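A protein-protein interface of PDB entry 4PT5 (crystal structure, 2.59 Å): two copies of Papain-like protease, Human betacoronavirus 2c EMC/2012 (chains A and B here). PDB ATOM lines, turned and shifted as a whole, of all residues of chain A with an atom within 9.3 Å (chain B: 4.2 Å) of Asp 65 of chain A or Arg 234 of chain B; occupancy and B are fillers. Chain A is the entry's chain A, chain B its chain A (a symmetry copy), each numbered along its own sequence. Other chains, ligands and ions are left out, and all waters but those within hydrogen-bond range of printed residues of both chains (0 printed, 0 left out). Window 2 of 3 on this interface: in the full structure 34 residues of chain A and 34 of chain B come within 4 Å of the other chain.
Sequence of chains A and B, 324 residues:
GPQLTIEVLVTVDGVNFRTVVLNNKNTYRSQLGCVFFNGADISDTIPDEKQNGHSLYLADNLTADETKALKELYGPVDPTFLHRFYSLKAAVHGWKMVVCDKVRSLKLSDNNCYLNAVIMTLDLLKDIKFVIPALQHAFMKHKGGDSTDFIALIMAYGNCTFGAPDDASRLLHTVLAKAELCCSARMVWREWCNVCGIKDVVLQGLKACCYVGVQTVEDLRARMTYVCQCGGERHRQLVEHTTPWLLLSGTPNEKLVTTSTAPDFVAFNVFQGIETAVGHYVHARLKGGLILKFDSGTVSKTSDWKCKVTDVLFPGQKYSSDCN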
ATOM      1  N   VAL A  12      24.420  19.374  26.545  1.00  0.00           N
ATOM      2  CA  VAL A  12      25.340  20.021  27.483  1.00  0.00           C
ATOM      3  C   VAL A  12      25.127  21.535  27.499  1.00  0.00           C
ATOM      4  O   VAL A  12      25.768  22.249  28.276  1.00  0.00           O
ATOM      5  CB  VAL A  12      26.831  19.715  27.180  1.00  0.00           C
ATOM      6  CG1 VAL A  12      27.132  18.235  27.362  1.00  0.00           C
ATOM      7  CG2 VAL A  12      27.230  20.193  25.785  1.00  0.00           C
ATOM      8  N   ASP A  13      24.226  22.014  26.638  1.00  0.00           N
ATOM      9  CA  ASP A  13      24.022  23.451  26.453  1.00  0.00           C
ATOM     10  C   ASP A  13      22.559  23.887  26.358  1.00  0.00           C
ATOM     11  O   ASP A  13      22.263  25.082  26.421  1.00  0.00           O
ATOM     12  CB  ASP A  13      24.818  23.958  25.236  1.00  0.00           C
ATOM     13  CG  ASP A  13      24.419  23.281  23.924  1.00  0.00           C
ATOM     14  OD1 ASP A  13      23.482  22.451  23.908  1.00  0.00           O
ATOM     15  OD2 ASP A  13      25.059  23.592  22.896  1.00  0.00           O
ATOM     16  N   ASN A  16      21.739  22.071  21.539  1.00  0.00           N
ATOM     17  CA  ASN A  16      21.985  20.881  20.718  1.00  0.00           C
ATOM     18  C   ASN A  16      21.691  19.594  21.478  1.00  0.00           C
ATOM     19  O   ASN A  16      22.101  19.439  22.633  1.00  0.00           O
ATOM     20  CB  ASN A  16      23.423  20.873  20.194  1.00  0.00           C
ATOM     21  CG  ASN A  16      23.762  22.125  19.409  1.00  0.00           C
ATOM     22  OD1 ASN A  16      23.486  22.216  18.212  1.00  0.00           O
ATOM     23  ND2 ASN A  16      24.367  23.102  20.085  1.00  0.00           N
ATOM     24  N   PHE A  17      20.978  18.681  20.822  1.00  0.00           N
ATOM     25  CA  PHE A  17      20.544  17.432  21.443  1.00  0.00           C
ATOM     26  C   PHE A  17      20.873  16.227  20.572  1.00  0.00           C
ATOM     27  O   PHE A  17      20.733  16.281  19.349  1.00  0.00           O
ATOM     28  CB  PHE A  17      19.035  17.459  21.698  1.00  0.00           C
ATOM     29  CG  PHE A  17      18.600  18.484  22.706  1.00  0.00           C
ATOM     30  CD1 PHE A  17      18.390  19.807  22.331  1.00  0.00           C
ATOM     31  CD2 PHE A  17      18.369  18.120  24.028  1.00  0.00           C
ATOM     32  CE1 PHE A  17      17.981  20.751  23.261  1.00  0.00           C
ATOM     33  CE2 PHE A  17      17.955  19.058  24.961  1.00  0.00           C
ATOM     34  CZ  PHE A  17      17.760  20.375  24.578  1.00  0.00           C
ATOM     35  N   ARG A  18      21.311  15.143  21.210  1.00  0.00           N
ATOM     36  CA  ARG A  18      21.489  13.856  20.536  1.00  0.00           C
ATOM     37  C   ARG A  18      20.641  12.778  21.201  1.00  0.00           C
ATOM     38  O   ARG A  18      20.389  12.834  22.409  1.00  0.00           O
ATOM     39  CB  ARG A  18      22.965  13.442  20.485  1.00  0.00           C
ATOM     40  CG  ARG A  18      23.642  13.250  21.833  1.00  0.00           C
ATOM     41  CD  ARG A  18      25.118  12.964  21.630  1.00  0.00           C
ATOM     42  NE  ARG A  18      25.874  12.945  22.881  1.00  0.00           N
ATOM     43  CZ  ARG A  18      26.190  11.844  23.558  1.00  0.00           C
ATOM     44  NH1 ARG A  18      25.814  10.646  23.125  1.00  0.00           N
ATOM     45  NH2 ARG A  18      26.888  11.942  24.678  1.00  0.00           N
ATOM     46  N   THR A  19      20.193  11.809  20.407  1.00  0.00           N
ATOM     47  CA  THR A  19      19.345  10.736  20.919  1.00  0.00           C
ATOM     48  C   THR A  19      20.175   9.493  21.240  1.00  0.00           C
ATOM     49  O   THR A  19      20.952   9.015  20.408  1.00  0.00           O
ATOM     50  CB  THR A  19      18.198  10.394  19.942  1.00  0.00           C
ATOM     51  OG1 THR A  19      17.567  11.604  19.504  1.00  0.00           O
ATOM     52  CG2 THR A  19      17.156   9.508  20.619  1.00  0.00           C
ATOM     53  N   VAL A  20      20.012   8.991  22.462  1.00  0.00           N
ATOM     54  CA  VAL A  20      20.740   7.811  22.922  1.00  0.00           C
ATOM     55  C   VAL A  20      19.751   6.741  23.385  1.00  0.00           C
ATOM     56  O   VAL A  20      18.838   7.026  24.161  1.00  0.00           O
ATOM     57  CB  VAL A  20      21.732   8.157  24.058  1.00  0.00           C
ATOM     58  CG1 VAL A  20      22.578   6.947  24.431  1.00  0.00           C
ATOM     59  CG2 VAL A  20      22.635   9.313  23.652  1.00  0.00           C
ATOM     60  N   VAL A  21      19.941   5.518  22.893  1.00  0.00           N
ATOM     61  CA  VAL A  21      19.098   4.374  23.249  1.00  0.00           C
ATOM     62  C   VAL A  21      19.717   3.604  24.422  1.00  0.00           C
ATOM     63  O   VAL A  21      20.842   3.109  24.327  1.00  0.00           O
ATOM     64  CB  VAL A  21      18.875   3.441  22.034  1.00  0.00           C
ATOM     65  CG1 VAL A  21      18.056   2.219  22.422  1.00  0.00           C
ATOM     66  CG2 VAL A  21      18.191   4.193  20.899  1.00  0.00           C
ATOM     67  N   ASN A  61      32.205  12.030  29.437  1.00  0.00           N
ATOM     68  CA  ASN A  61      32.283  11.340  28.143  1.00  0.00           C
ATOM     69  C   ASN A  61      31.664  12.121  26.982  1.00  0.00           C
ATOM     70  O   ASN A  61      30.924  11.566  26.167  1.00  0.00           O
ATOM     71  CB  ASN A  61      31.660   9.943  28.238  1.00  0.00           C
ATOM     72  CG  ASN A  61      32.293   9.093  29.320  1.00  0.00           C
ATOM     73  OD1 ASN A  61      33.498   8.834  29.302  1.00  0.00           O
ATOM     74  ND2 ASN A  61      31.481   8.649  30.272  1.00  0.00           N
ATOM     75  N   LEU A  62      31.971  13.412  26.918  1.00  0.00           N
ATOM     76  CA  LEU A  62      31.417  14.270  25.882  1.00  0.00           C
ATOM     77  C   LEU A  62      31.972  13.901  24.510  1.00  0.00           C
ATOM     78  O   LEU A  62      33.151  13.563  24.368  1.00  0.00           O
ATOM     79  CB  LEU A  62      31.697  15.748  26.176  1.00  0.00           C
ATOM     80  CG  LEU A  62      31.398  16.365  27.547  1.00  0.00           C
ATOM     81  CD1 LEU A  62      31.450  17.879  27.424  1.00  0.00           C
ATOM     82  CD2 LEU A  62      30.058  15.929  28.120  1.00  0.00           C
ATOM     83  N   THR A  63      31.104  13.960  23.507  1.00  0.00           N
ATOM     84  CA  THR A  63      31.503  13.743  22.123  1.00  0.00           C
ATOM     85  C   THR A  63      32.292  14.955  21.621  1.00  0.00           C
ATOM     86  O   THR A  63      32.229  16.031  22.222  1.00  0.00           O
ATOM     87  CB  THR A  63      30.277  13.492  21.228  1.00  0.00           C
ATOM     88  OG1 THR A  63      29.328  14.552  21.403  1.00  0.00           O
ATOM     89  CG2 THR A  63      29.614  12.171  21.592  1.00  0.00           C
ATOM     90  N   ALA A  64      33.042  14.775  20.535  1.00  0.00           N
ATOM     91  CA  ALA A  64      33.834  15.857  19.948  1.00  0.00           C
ATOM     92  C   ALA A  64      32.993  17.114  19.730  1.00  0.00           C
ATOM     93  O   ALA A  64      33.441  18.227  20.014  1.00  0.00           O
ATOM     94  CB  ALA A  64      34.469  15.405  18.643  1.00  0.00           C
ATOM     95  N   ASP A  65      31.768  16.914  19.241  1.00  0.00           N
ATOM     96  CA  ASP A  65      30.806  17.995  19.025  1.00  0.00           C
ATOM     97  C   ASP A  65      30.357  18.659  20.328  1.00  0.00           C
ATOM     98  O   ASP A  65      30.179  19.878  20.378  1.00  0.00           O
ATOM     99  CB  ASP A  65      29.585  17.478  18.254  1.00  0.00           C
ATOM    100  CG  ASP A  65      29.911  17.097  16.817  1.00  0.00           C
ATOM    101  OD1 ASP A  65      31.055  17.335  16.368  1.00  0.00           O
ATOM    102  OD2 ASP A  65      29.014  16.556  16.132  1.00  0.00           O
ATOM    103  N   GLU A  66      30.173  17.853  21.374  1.00  0.00           N
ATOM    104  CA  GLU A  66      29.780  18.360  22.690  1.00  0.00           C
ATOM    105  C   GLU A  66      30.907  19.142  23.366  1.00  0.00           C
ATOM    106  O   GLU A  66      30.661  20.194  23.954  1.00  0.00           O
ATOM    107  CB  GLU A  66      29.300  17.219  23.592  1.00  0.00           C
ATOM    108  CG  GLU A  66      27.869  16.784  23.312  1.00  0.00           C
ATOM    109  CD  GLU A  66      27.465  15.526  24.060  1.00  0.00           C
ATOM    110  OE1 GLU A  66      28.346  14.703  24.394  1.00  0.00           O
ATOM    111  OE2 GLU A  66      26.250  15.353  24.304  1.00  0.00           O
ATOM    112  N   THR A  67      32.133  18.628  23.266  1.00  0.00           N
ATOM    113  CA  THR A  67      33.320  19.290  23.816  1.00  0.00           C
ATOM    114  C   THR A  67      33.537  20.674  23.196  1.00  0.00           C
ATOM    115  O   THR A  67      33.831  21.639  23.909  1.00  0.00           O
ATOM    116  CB  THR A  67      34.584  18.415  23.641  1.00  0.00           C
ATOM    117  OG1 THR A  67      34.435  17.201  24.388  1.00  0.00           O
ATOM    118  CG2 THR A  67      35.837  19.141  24.117  1.00  0.00           C
ATOM    119  N   LYS A  68      33.379  20.765  21.875  1.00  0.00           N
ATOM    120  CA  LYS A  68      33.571  22.023  21.151  1.00  0.00           C
ATOM    121  C   LYS A  68      32.509  23.061  21.519  1.00  0.00           C
ATOM    122  O   LYS A  68      32.832  24.223  21.772  1.00  0.00           O
ATOM    123  CB  LYS A  68      33.606  21.788  19.634  1.00  0.00           C
ATOM    124  CG  LYS A  68      33.954  23.031  18.828  1.00  0.00           C
ATOM    125  CD  LYS A  68      34.342  22.704  17.395  1.00  0.00           C
ATOM    126  CE  LYS A  68      34.777  23.963  16.656  1.00  0.00           C
ATOM    127  NZ  LYS A  68      35.265  23.683  15.275  1.00  0.00           N
ATOM    128  N   ALA A  69      31.250  22.629  21.556  1.00  0.00           N
ATOM    129  CA  ALA A  69      30.132  23.497  21.917  1.00  0.00           C
ATOM    130  C   ALA A  69      30.204  23.932  23.379  1.00  0.00           C
ATOM    131  O   ALA A  69      29.795  25.042  23.722  1.00  0.00           O
ATOM    132  CB  ALA A  69      28.809  22.803  21.632  1.00  0.00           C
ATOM    133  N   LEU A  70      30.728  23.049  24.229  1.00  0.00           N
ATOM    134  CA  LEU A  70      30.955  23.346  25.642  1.00  0.00           C
ATOM    135  C   LEU A  70      31.998  24.449  25.800  1.00  0.00           C
ATOM    136  O   LEU A  70      31.873  25.307  26.673  1.00  0.00           O
ATOM    137  CB  LEU A  70      31.397  22.076  26.386  1.00  0.00           C
ATOM    138  CG  LEU A  70      31.637  21.996  27.903  1.00  0.00           C
ATOM    139  CD1 LEU A  70      33.027  22.482  28.298  1.00  0.00           C
ATOM    140  CD2 LEU A  70      30.555  22.707  28.705  1.00  0.00           C
ATOM    141  N   LYS A  71      33.020  24.411  24.947  1.00  0.00           N
ATOM    142  CA  LYS A  71      34.105  25.388  24.970  1.00  0.00           C
ATOM    143  C   LYS A  71      33.647  26.764  24.477  1.00  0.00           C
ATOM    144  O   LYS A  71      34.023  27.787  25.046  1.00  0.00           O
ATOM    145  CB  LYS A  71      35.289  24.886  24.138  1.00  0.00           C
ATOM    146  CG  LYS A  71      36.569  25.692  24.303  1.00  0.00           C
ATOM    147  CD  LYS A  71      37.726  25.049  23.552  1.00  0.00           C
ATOM    148  CE  LYS A  71      38.987  25.897  23.626  1.00  0.00           C
ATOM    149  NZ  LYS A  71      38.886  27.127  22.791  1.00  0.00           N
ATOM    150  N   GLU A  72      32.832  26.783  23.425  1.00  0.00           N
ATOM    151  CA  GLU A  72      32.361  28.039  22.841  1.00  0.00           C
ATOM    152  C   GLU A  72      31.352  28.771  23.721  1.00  0.00           C
ATOM    153  O   GLU A  72      31.243  29.996  23.658  1.00  0.00           O
ATOM    154  CB  GLU A  72      31.783  27.803  21.444  1.00  0.00           C
ATOM    155  CG  GLU A  72      32.848  27.643  20.365  1.00  0.00           C
ATOM    156  CD  GLU A  72      32.310  27.065  19.067  1.00  0.00           C
ATOM    157  OE1 GLU A  72      31.128  26.659  19.020  1.00  0.00           O
ATOM    158  OE2 GLU A  72      33.082  27.013  18.085  1.00  0.00           O
ATOM    159  N   LEU A  73      30.627  28.018  24.544  1.00  0.00           N
ATOM    160  CA  LEU A  73      29.608  28.587  25.423  1.00  0.00           C
ATOM    161  C   LEU A  73      30.175  29.061  26.762  1.00  0.00           C
ATOM    162  O   LEU A  73      29.853  30.161  27.217  1.00  0.00           O
ATOM    163  CB  LEU A  73      28.472  27.582  25.649  1.00  0.00           C
ATOM    164  CG  LEU A  73      27.339  27.954  26.612  1.00  0.00           C
ATOM    165  CD1 LEU A  73      26.541  29.158  26.127  1.00  0.00           C
ATOM    166  CD2 LEU A  73      26.424  26.762  26.821  1.00  0.00           C
ATOM    167  N   GLU B 191      35.244   8.739  15.663  1.00  0.00           N
ATOM    168  CA  GLU B 191      33.798   8.878  15.567  1.00  0.00           C
ATOM    169  C   GLU B 191      33.389   8.522  14.149  1.00  0.00           C
ATOM    170  O   GLU B 191      33.927   9.082  13.189  1.00  0.00           O
ATOM    171  CB  GLU B 191      33.366  10.306  15.904  1.00  0.00           C
ATOM    172  CG  GLU B 191      33.723  10.760  17.312  1.00  0.00           C
ATOM    173  CD  GLU B 191      33.031  12.050  17.712  1.00  0.00           C
ATOM    174  OE1 GLU B 191      32.678  12.850  16.817  1.00  0.00           O
ATOM    175  OE2 GLU B 191      32.841  12.265  18.930  1.00  0.00           O
ATOM    176  N   TRP B 192      32.453   7.585  14.008  1.00  0.00           N
ATOM    177  CA  TRP B 192      32.058   7.116  12.679  1.00  0.00           C
ATOM    178  C   TRP B 192      30.632   6.657  12.553  1.00  0.00           C
ATOM    179  O   TRP B 192      29.970   6.330  13.542  1.00  0.00           O
ATOM    180  CB  TRP B 192      33.019   6.029  12.175  1.00  0.00           C
ATOM    181  CG  TRP B 192      32.737   4.636  12.699  1.00  0.00           C
ATOM    182  CD1 TRP B 192      32.006   3.628  12.074  1.00  0.00           C
ATOM    183  CD2 TRP B 192      33.179   4.048  13.973  1.00  0.00           C
ATOM    184  NE1 TRP B 192      31.962   2.497  12.851  1.00  0.00           N
ATOM    185  CE2 TRP B 192      32.645   2.679  14.000  1.00  0.00           C
ATOM    186  CE3 TRP B 192      33.933   4.501  15.053  1.00  0.00           C
ATOM    187  CZ2 TRP B 192      32.871   1.821  15.069  1.00  0.00           C
ATOM    188  CZ3 TRP B 192      34.150   3.626  16.126  1.00  0.00           C
ATOM    189  CH2 TRP B 192      33.632   2.320  16.132  1.00  0.00           C
ATOM    190  N   MET B 224      31.210   3.356  22.181  1.00  0.00           N
ATOM    191  CA  MET B 224      30.019   4.125  22.533  1.00  0.00           C
ATOM    192  C   MET B 224      29.099   4.231  21.315  1.00  0.00           C
ATOM    193  O   MET B 224      29.563   4.499  20.206  1.00  0.00           O
ATOM    194  CB  MET B 224      30.427   5.516  23.029  1.00  0.00           C
ATOM    195  CG  MET B 224      29.280   6.410  23.475  1.00  0.00           C
ATOM    196  SD  MET B 224      28.510   5.893  25.023  1.00  0.00           S
ATOM    197  CE  MET B 224      27.072   6.963  25.034  1.00  0.00           C
ATOM    198  N   THR B 225      27.800   4.020  21.526  1.00  0.00           N
ATOM    199  CA  THR B 225      26.826   4.030  20.432  1.00  0.00           C
ATOM    200  C   THR B 225      25.627   4.945  20.717  1.00  0.00           C
ATOM    201  O   THR B 225      25.020   4.875  21.787  1.00  0.00           O
ATOM    202  CB  THR B 225      26.344   2.597  20.093  1.00  0.00           C
ATOM    203  OG1 THR B 225      27.464   1.797  19.689  1.00  0.00           O
ATOM    204  CG2 THR B 225      25.313   2.604  18.965  1.00  0.00           C
ATOM    205  N   TYR B 226      25.312   5.806  19.749  1.00  0.00           N
ATOM    206  CA  TYR B 226      24.111   6.649  19.789  1.00  0.00           C
ATOM    207  C   TYR B 226      23.570   6.896  18.373  1.00  0.00           C
ATOM    208  O   TYR B 226      24.223   6.542  17.391  1.00  0.00           O
ATOM    209  CB  TYR B 226      24.378   7.972  20.529  1.00  0.00           C
ATOM    210  CG  TYR B 226      25.430   8.862  19.900  1.00  0.00           C
ATOM    211  CD1 TYR B 226      26.784   8.689  20.185  1.00  0.00           C
ATOM    212  CD2 TYR B 226      25.068   9.892  19.031  1.00  0.00           C
ATOM    213  CE1 TYR B 226      27.747   9.506  19.614  1.00  0.00           C
ATOM    214  CE2 TYR B 226      26.026  10.713  18.451  1.00  0.00           C
ATOM    215  CZ  TYR B 226      27.361  10.516  18.746  1.00  0.00           C
ATOM    216  OH  TYR B 226      28.310  11.330  18.176  1.00  0.00           O
ATOM    217  N   CYS B 228      22.523   8.432  14.821  1.00  0.00           N
ATOM    218  CA  CYS B 228      23.191   9.295  13.845  1.00  0.00           C
ATOM    219  C   CYS B 228      22.259  10.334  13.213  1.00  0.00           C
ATOM    220  O   CYS B 228      21.031  10.224  13.296  1.00  0.00           O
ATOM    221  CB  CYS B 228      23.835   8.447  12.742  1.00  0.00           C
ATOM    222  SG  CYS B 228      24.809   9.394  11.544  1.00  0.00           S
ATOM    223  N   GLU B 233      23.215   4.722  13.003  1.00  0.00           N
ATOM    224  CA  GLU B 233      23.929   4.638  14.277  1.00  0.00           C
ATOM    225  C   GLU B 233      25.325   5.254  14.202  1.00  0.00           C
ATOM    226  O   GLU B 233      26.071   5.016  13.248  1.00  0.00           O
ATOM    227  CB  GLU B 233      24.017   3.186  14.758  1.00  0.00           C
ATOM    228  CG  GLU B 233      22.768   2.681  15.466  1.00  0.00           C
ATOM    229  CD  GLU B 233      22.869   1.224  15.882  1.00  0.00           C
ATOM    230  OE1 GLU B 233      22.461   0.902  17.017  1.00  0.00           O
ATOM    231  OE2 GLU B 233      23.354   0.396  15.080  1.00  0.00           O
ATOM    232  N   ARG B 234      25.660   6.053  15.214  1.00  0.00           N
ATOM    233  CA  ARG B 234      26.998   6.625  15.363  1.00  0.00           C
ATOM    234  C   ARG B 234      27.772   5.926  16.468  1.00  0.00           C
ATOM    235  O   ARG B 234      27.203   5.536  17.492  1.00  0.00           O
ATOM    236  CB  ARG B 234      26.933   8.127  15.655  1.00  0.00           C
ATOM    237  CG  ARG B 234      26.951   9.003  14.416  1.00  0.00           C
ATOM    238  CD  ARG B 234      27.255  10.452  14.754  1.00  0.00           C
ATOM    239  NE  ARG B 234      28.694  10.703  14.804  1.00  0.00           N
ATOM    240  CZ  ARG B 234      29.249  11.891  15.045  1.00  0.00           C
ATOM    241  NH1 ARG B 234      28.493  12.965  15.263  1.00  0.00           N
ATOM    242  NH2 ARG B 234      30.569  12.009  15.071  1.00  0.00           N
ATOM    243  N   HIS B 235      29.075   5.781  16.255  1.00  0.00           N
ATOM    244  CA  HIS B 235      29.945   5.118  17.215  1.00  0.00           C
ATOM    245  C   HIS B 235      31.132   5.965  17.568  1.00  0.00           C
ATOM    246  O   HIS B 235      31.698   6.648  16.714  1.00  0.00           O
ATOM    247  CB  HIS B 235      30.412   3.769  16.680  1.00  0.00           C
ATOM    248  CG  HIS B 235      29.290   2.862  16.234  1.00  0.00           C
ATOM    249  ND1 HIS B 235      28.480   2.230  17.102  1.00  0.00           N
ATOM    250  CD2 HIS B 235      28.871   2.488  14.960  1.00  0.00           C
ATOM    251  CE1 HIS B 235      27.583   1.491  16.422  1.00  0.00           C
ATOM    252  NE2 HIS B 235      27.824   1.650  15.111  1.00  0.00           N
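OD2 of Asp 65 of chain A lies within salt-bridge range of NH1 of Arg 234 of chain B, at 3.7 Å. The side-chain carboxylate (OE2) of Glu 191 of chain B lies within hydrogen-bond range of the backbone NH (N) of Ala 64 of chain A, at 3.0 Å.
N of Thr 63 of chain A lies within hydrogen-bond range of OE1 of Glu 66 of chain A (3.0 Å). OG1 of Thr 67 of chain A lies within hydrogen-bond range of O of Thr 63 of chain A (3.3 Å). N of Arg 234 of chain B lies within hydrogen-bond range of O of Tyr 226 of chain B, 2.7 Å away. The side-chain carboxylate (OE1) of Glu 191 of chain B lies within salt-bridge range of the guanidinium group (NH2) of Arg 234 of chain B (2.9 Å). The guanidinium group of Arg 18 of chain A is in salt-bridge range of the side-chain carboxylate of Glu 66 of chain A (2.8 Å).
Among the printed residues, merely in contact across the chains: Arg 18 of chain A with Tyr 226 of chain B, Thr 19 of chain A with Tyr 226 of chain B, Val 20 of chain A with Tyr 226 of chain B, Thr 63 of chain A with Glu 191 of chain B and Thr 63 of chain A with Tyr 226 of chain B.
Of the printed residues of chain B, Thr 63 of chain A touches Glu 191 (3.7 Å) and Tyr 226 (3.8 Å). Of the printed residues of chain B, Ala 64 of chain A touches Glu 191 (3.0 Å). Of chain B, only Arg 234 (3.7 Å) comes within 4 Å of Asp 65 of chain A. Glu 66 of chain A touches none of the printed residues of chain B. No residue of chain A comes within 4 Å of Thr 225 of chain B. Of chain A, only Arg 18 (3.7 Å), Thr 19 (3.6 Å), Val 20 (3.8 Å) and Thr 63 (3.8 Å) come within 4 Å of Tyr 226 of chain B. Printed residues of chain A within 4 Å of Arg 234 of chain B: Asp 65. His 235 of chain B touches none of the printed residues of chain A.
Of the 9 printed residues of chain B, 3 touch a printed residue of chain A. Among the printed residues, 7 pairs touch across the chains.
No position is printed for both chains. Of the 7 pairs that touch across the chains among the printed residues, none has its exchanged pair printed and touching as well.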
